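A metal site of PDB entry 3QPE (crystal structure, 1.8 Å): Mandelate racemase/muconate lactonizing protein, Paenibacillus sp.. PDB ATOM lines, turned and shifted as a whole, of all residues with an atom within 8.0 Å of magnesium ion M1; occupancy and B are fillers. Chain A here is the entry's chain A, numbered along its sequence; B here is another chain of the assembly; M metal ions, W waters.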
ATOM      1  N   ASN A 209      20.663  10.721  30.394  1.00  0.00           N
ATOM      2  CA  ASN A 209      19.795  10.022  29.448  1.00  0.00           C
ATOM      3  C   ASN A 209      18.341  10.045  29.908  1.00  0.00           C
ATOM      4  O   ASN A 209      17.631   9.036  29.849  1.00  0.00           O
ATOM      5  CB  ASN A 209      20.275   8.605  29.149  1.00  0.00           C
ATOM      6  CG  ASN A 209      21.575   8.592  28.362  1.00  0.00           C
ATOM      7  OD1 ASN A 209      22.648   8.386  28.932  1.00  0.00           O
ATOM      8  ND2 ASN A 209      21.499   8.826  27.056  1.00  0.00           N
ATOM      9  N   ASN A 210      17.928  11.229  30.366  1.00  0.00           N
ATOM     10  CA  ASN A 210      16.527  11.521  30.658  1.00  0.00           C
ATOM     11  C   ASN A 210      16.000  10.790  31.873  1.00  0.00           C
ATOM     12  O   ASN A 210      14.793  10.788  32.133  1.00  0.00           O
ATOM     13  CB  ASN A 210      15.661  11.256  29.431  1.00  0.00           C
ATOM     14  CG  ASN A 210      15.845  12.315  28.354  1.00  0.00           C
ATOM     15  OD1 ASN A 210      16.276  13.425  28.636  1.00  0.00           O
ATOM     16  ND2 ASN A 210      15.541  11.970  27.110  1.00  0.00           N
ATOM     17  N   GLU A 233      23.645  17.236  30.728  1.00  0.00           N
ATOM     18  CA  GLU A 233      23.104  16.763  29.468  1.00  0.00           C
ATOM     19  C   GLU A 233      21.901  15.848  29.663  1.00  0.00           C
ATOM     20  O   GLU A 233      21.971  14.868  30.409  1.00  0.00           O
ATOM     21  CB  GLU A 233      24.212  16.040  28.687  1.00  0.00           C
ATOM     22  CG  GLU A 233      23.736  15.190  27.507  1.00  0.00           C
ATOM     23  CD  GLU A 233      24.881  14.767  26.605  1.00  0.00           C
ATOM     24  OE1 GLU A 233      26.011  15.257  26.745  1.00  0.00           O
ATOM     25  OE2 GLU A 233      24.623  13.959  25.711  1.00  0.00           O
ATOM     26  N   GLU A 234      20.795  16.170  29.014  1.00  0.00           N
ATOM     27  CA  GLU A 234      19.575  15.353  29.077  1.00  0.00           C
ATOM     28  C   GLU A 234      19.181  14.899  30.487  1.00  0.00           C
ATOM     29  O   GLU A 234      18.958  13.713  30.726  1.00  0.00           O
ATOM     30  CB  GLU A 234      19.676  14.144  28.144  1.00  0.00           C
ATOM     31  CG  GLU A 234      19.803  14.519  26.667  1.00  0.00           C
ATOM     32  CD  GLU A 234      19.177  13.463  25.734  1.00  0.00           C
ATOM     33  OE1 GLU A 234      19.592  12.295  25.759  1.00  0.00           O
ATOM     34  OE2 GLU A 234      18.263  13.803  24.985  1.00  0.00           O
ATOM     35  N   ALA A 235      19.058  15.838  31.421  1.00  0.00           N
ATOM     36  CA  ALA A 235      18.592  15.508  32.758  1.00  0.00           C
ATOM     37  C   ALA A 235      17.236  14.792  32.649  1.00  0.00           C
ATOM     38  O   ALA A 235      16.985  13.820  33.336  1.00  0.00           O
ATOM     39  CB  ALA A 235      18.455  16.769  33.608  1.00  0.00           C
ATOM     40  N   PHE A 236      16.391  15.297  31.764  1.00  0.00           N
ATOM     41  CA  PHE A 236      15.038  14.789  31.565  1.00  0.00           C
ATOM     42  C   PHE A 236      14.621  15.271  30.168  1.00  0.00           C
ATOM     43  O   PHE A 236      15.270  16.160  29.589  1.00  0.00           O
ATOM     44  CB  PHE A 236      14.085  15.343  32.629  1.00  0.00           C
ATOM     45  CG  PHE A 236      14.343  16.775  32.973  1.00  0.00           C
ATOM     46  CD1 PHE A 236      14.956  17.112  34.159  1.00  0.00           C
ATOM     47  CD2 PHE A 236      14.012  17.781  32.082  1.00  0.00           C
ATOM     48  CE1 PHE A 236      15.226  18.432  34.468  1.00  0.00           C
ATOM     49  CE2 PHE A 236      14.270  19.095  32.390  1.00  0.00           C
ATOM     50  CZ  PHE A 236      14.874  19.434  33.577  1.00  0.00           C
ATOM     51  N   HIS A 237      13.590  14.671  29.572  1.00  0.00           N
ATOM     52  CA  HIS A 237      13.277  15.066  28.215  1.00  0.00           C
ATOM     53  C   HIS A 237      12.998  16.568  28.170  1.00  0.00           C
ATOM     54  O   HIS A 237      12.250  17.077  28.998  1.00  0.00           O
ATOM     55  CB  HIS A 237      12.075  14.300  27.658  1.00  0.00           C
ATOM     56  CG  HIS A 237      11.767  14.669  26.247  1.00  0.00           C
ATOM     57  ND1 HIS A 237      12.672  14.508  25.227  1.00  0.00           N
ATOM     58  CD2 HIS A 237      10.671  15.260  25.694  1.00  0.00           C
ATOM     59  CE1 HIS A 237      12.140  14.944  24.095  1.00  0.00           C
ATOM     60  NE2 HIS A 237      10.933  15.407  24.348  1.00  0.00           N
ATOM     61  N   GLU A 238      13.594  17.254  27.200  1.00  0.00           N
ATOM     62  CA  GLU A 238      13.529  18.707  27.133  1.00  0.00           C
ATOM     63  C   GLU A 238      12.108  19.267  27.253  1.00  0.00           C
ATOM     64  O   GLU A 238      11.176  18.787  26.619  1.00  0.00           O
ATOM     65  CB  GLU A 238      14.220  19.254  25.880  1.00  0.00           C
ATOM     66  CG  GLU A 238      13.719  18.655  24.576  1.00  0.00           C
ATOM     67  CD  GLU A 238      14.585  17.499  24.124  1.00  0.00           C
ATOM     68  OE1 GLU A 238      14.761  17.301  22.908  1.00  0.00           O
ATOM     69  OE2 GLU A 238      15.094  16.804  25.024  1.00  0.00           O
ATOM     70  N   ASP A 239      11.991  20.305  28.064  1.00  0.00           N
ATOM     71  CA  ASP A 239      10.722  20.916  28.438  1.00  0.00           C
ATOM     72  C   ASP A 239      11.080  22.352  28.816  1.00  0.00           C
ATOM     73  O   ASP A 239      11.869  22.578  29.732  1.00  0.00           O
ATOM     74  CB  ASP A 239      10.132  20.157  29.627  1.00  0.00           C
ATOM     75  CG  ASP A 239       8.813  20.730  30.110  1.00  0.00           C
ATOM     76  OD1 ASP A 239       8.648  21.966  30.074  1.00  0.00           O
ATOM     77  OD2 ASP A 239       7.938  19.933  30.545  1.00  0.00           O
ATOM     78  N   TYR A 243      13.317  23.635  32.159  1.00  0.00           N
ATOM     79  CA  TYR A 243      14.646  24.204  32.005  1.00  0.00           C
ATOM     80  C   TYR A 243      14.688  25.674  32.431  1.00  0.00           C
ATOM     81  O   TYR A 243      15.698  26.148  32.936  1.00  0.00           O
ATOM     82  CB  TYR A 243      15.164  24.045  30.584  1.00  0.00           C
ATOM     83  CG  TYR A 243      15.816  22.699  30.295  1.00  0.00           C
ATOM     84  CD1 TYR A 243      16.487  21.987  31.300  1.00  0.00           C
ATOM     85  CD2 TYR A 243      15.776  22.153  29.016  1.00  0.00           C
ATOM     86  CE1 TYR A 243      17.080  20.749  31.029  1.00  0.00           C
ATOM     87  CE2 TYR A 243      16.382  20.939  28.731  1.00  0.00           C
ATOM     88  CZ  TYR A 243      17.033  20.235  29.731  1.00  0.00           C
ATOM     89  OH  TYR A 243      17.615  19.043  29.404  1.00  0.00           O
ATOM     90  N   ALA A 260      22.830  21.100  28.323  1.00  0.00           N
ATOM     91  CA  ALA A 260      23.054  20.507  27.007  1.00  0.00           C
ATOM     92  C   ALA A 260      21.925  19.542  26.665  1.00  0.00           C
ATOM     93  O   ALA A 260      21.441  18.804  27.514  1.00  0.00           O
ATOM     94  CB  ALA A 260      24.399  19.772  26.998  1.00  0.00           C
ATOM     95  N   ASP A 261      21.505  19.522  25.402  1.00  0.00           N
ATOM     96  CA  ASP A 261      20.414  18.665  24.979  1.00  0.00           C
ATOM     97  C   ASP A 261      20.351  18.606  23.445  1.00  0.00           C
ATOM     98  O   ASP A 261      21.066  19.329  22.792  1.00  0.00           O
ATOM     99  CB  ASP A 261      19.099  19.149  25.578  1.00  0.00           C
ATOM    100  CG  ASP A 261      18.180  17.999  25.929  1.00  0.00           C
ATOM    101  OD1 ASP A 261      18.183  17.011  25.183  1.00  0.00           O
ATOM    102  OD2 ASP A 261      17.466  18.072  26.957  1.00  0.00           O
ATOM    103  N   GLY A 262      19.537  17.716  22.881  1.00  0.00           N
ATOM    104  CA  GLY A 262      19.286  17.715  21.445  1.00  0.00           C
ATOM    105  C   GLY A 262      19.504  16.409  20.688  1.00  0.00           C
ATOM    106  O   GLY A 262      19.129  16.306  19.527  1.00  0.00           O
ATOM    107  N   GLU A 263      20.098  15.404  21.323  1.00  0.00           N
ATOM    108  CA  GLU A 263      20.289  14.118  20.621  1.00  0.00           C
ATOM    109  C   GLU A 263      18.968  13.366  20.406  1.00  0.00           C
ATOM    110  O   GLU A 263      17.967  13.637  21.080  1.00  0.00           O
ATOM    111  CB  GLU A 263      21.308  13.227  21.353  1.00  0.00           C
ATOM    112  CG  GLU A 263      20.736  12.527  22.575  1.00  0.00           C
ATOM    113  CD  GLU A 263      21.803  11.783  23.350  1.00  0.00           C
ATOM    114  OE1 GLU A 263      21.650  10.555  23.565  1.00  0.00           O
ATOM    115  OE2 GLU A 263      22.803  12.425  23.739  1.00  0.00           O
ATOM    116  N   GLY A 264      18.976  12.444  19.448  1.00  0.00           N
ATOM    117  CA  GLY A 264      17.815  11.599  19.190  1.00  0.00           C
ATOM    118  C   GLY A 264      16.592  12.338  18.689  1.00  0.00           C
ATOM    119  O   GLY A 264      16.699  13.268  17.893  1.00  0.00           O
ATOM    120  N   LEU A 265      15.413  11.945  19.179  1.00  0.00           N
ATOM    121  CA  LEU A 265      14.177  12.568  18.730  1.00  0.00           C
ATOM    122  C   LEU A 265      13.919  13.812  19.564  1.00  0.00           C
ATOM    123  O   LEU A 265      13.253  13.745  20.607  1.00  0.00           O
ATOM    124  CB  LEU A 265      13.005  11.596  18.878  1.00  0.00           C
ATOM    125  CG  LEU A 265      13.105  10.265  18.123  1.00  0.00           C
ATOM    126  CD1 LEU A 265      12.072   9.286  18.632  1.00  0.00           C
ATOM    127  CD2 LEU A 265      12.963  10.512  16.624  1.00  0.00           C
ATOM    128  N   ALA A 266      14.485  14.937  19.122  1.00  0.00           N
ATOM    129  CA  ALA A 266      14.414  16.187  19.895  1.00  0.00           C
ATOM    130  C   ALA A 266      13.063  16.883  19.748  1.00  0.00           C
ATOM    131  O   ALA A 266      12.385  16.728  18.741  1.00  0.00           O
ATOM    132  CB  ALA A 266      15.530  17.130  19.482  1.00  0.00           C
ATOM    133  N   SER A 267      12.674  17.668  20.758  1.00  0.00           N
ATOM    134  CA  SER A 267      11.545  18.551  20.598  1.00  0.00           C
ATOM    135  C   SER A 267      11.794  19.445  19.382  1.00  0.00           C
ATOM    136  O   SER A 267      12.874  19.974  19.218  1.00  0.00           O
ATOM    137  CB  SER A 267      11.360  19.416  21.834  1.00  0.00           C
ATOM    138  OG  SER A 267      10.573  20.550  21.521  1.00  0.00           O
ATOM    139  N   LEU A 270      13.197  22.913  20.402  1.00  0.00           N
ATOM    140  CA  LEU A 270      14.406  22.998  21.215  1.00  0.00           C
ATOM    141  C   LEU A 270      15.263  24.218  20.899  1.00  0.00           C
ATOM    142  O   LEU A 270      15.746  24.894  21.802  1.00  0.00           O
ATOM    143  CB  LEU A 270      15.257  21.724  21.031  1.00  0.00           C
ATOM    144  CG  LEU A 270      16.526  21.712  21.885  1.00  0.00           C
ATOM    145  CD1 LEU A 270      16.159  21.741  23.367  1.00  0.00           C
ATOM    146  CD2 LEU A 270      17.369  20.470  21.563  1.00  0.00           C
ATOM    147  N   GLN A 283      22.985  19.473  20.668  1.00  0.00           N
ATOM    148  CA  GLN A 283      23.726  18.219  20.482  1.00  0.00           C
ATOM    149  C   GLN A 283      23.195  17.273  19.389  1.00  0.00           C
ATOM    150  O   GLN A 283      23.313  16.044  19.498  1.00  0.00           O
ATOM    151  CB  GLN A 283      23.785  17.486  21.839  1.00  0.00           C
ATOM    152  CG  GLN A 283      24.480  18.298  22.904  1.00  0.00           C
ATOM    153  CD  GLN A 283      24.654  17.524  24.198  1.00  0.00           C
ATOM    154  OE1 GLN A 283      23.685  17.049  24.784  1.00  0.00           O
ATOM    155  NE2 GLN A 283      25.891  17.414  24.659  1.00  0.00           N
ATOM    156  N   HIS B 237       8.352  11.048  29.882  1.00  0.00           N
ATOM    157  CA  HIS B 237       8.221  11.198  28.429  1.00  0.00           C
ATOM    158  C   HIS B 237       8.291   9.825  27.780  1.00  0.00           C
ATOM    159  O   HIS B 237       9.150   9.024  28.122  1.00  0.00           O
ATOM    160  CB  HIS B 237       9.279  12.123  27.842  1.00  0.00           C
ATOM    161  CG  HIS B 237       9.142  12.317  26.363  1.00  0.00           C
ATOM    162  ND1 HIS B 237       8.056  12.940  25.779  1.00  0.00           N
ATOM    163  CD2 HIS B 237       9.966  11.960  25.338  1.00  0.00           C
ATOM    164  CE1 HIS B 237       8.216  12.957  24.468  1.00  0.00           C
ATOM    165  NE2 HIS B 237       9.360  12.373  24.173  1.00  0.00           N
HETATM  166 MG    MG M   1      16.762  15.373  24.936  1.00  0.00          MG
HETATM  167 MG    MG M   2      23.773  12.061  25.687  1.00  0.00          MG
HETATM  168  O   HOH W   1      15.138  13.773  24.673  1.00  0.00           O
HETATM  169  O   HOH W   2      16.941  15.672  22.772  1.00  0.00           O
HETATM  170  O   HOH W   3      16.370  15.463  27.096  1.00  0.00           O
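Three residues have an atom within 4 Å of magnesium ion M1: Glu 234, Glu 238 and Asp 261. Along chain A the residues within 4 Å of magnesium ion M1 span positions 234 to 261.
Water W2 lies within hydrogen-bond range of the side-chain carboxylate (OE1) of Glu 238 (2.7 Å), the backbone carbonyl oxygen (O) of Glu 263 (2.8 Å) and the backbone NH (N) of Gly 262 (3.3 Å). Water W1 bridges a ring nitrogen (ND1) of His 237 of chain A (2.6 Å) and the side-chain amide nitrogen of Asn 210 (3.1 Å).
Magnesium ion M1 is bound by OE2 of Glu 234, OD1 of Asp 261, water W2, water W3, OE2 of Glu 238 and water W1. Magnesium ion M1 has six donor atoms within binding distance.
The backbone carbonyl oxygen (O) of Glu 234 sits at hydrogen-bond distance from the backbone NH (N) of Asn 210, at 2.7 Å. N of Glu 234 sits at hydrogen-bond distance from O of Ala 260 (3.1 Å). N of Asn 209 sits at hydrogen-bond distance from O of Glu 234. The side-chain hydroxyl (OH) of Tyr 243 lies within hydrogen-bond range of the side-chain carboxylate (OD2) of Asp 261 (2.6 Å). The backbone NH (N) of Gln 283 is in hydrogen-bond range of the backbone carbonyl oxygen (O) of Asp 261, 2.9 Å away. A ring nitrogen (ND1) of His 237 of chain A lies close to the side-chain carboxylate (OE2) of Glu 238 (3.3 Å). N of Ser 267 is in hydrogen-bond range of OE1 of Glu 238.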
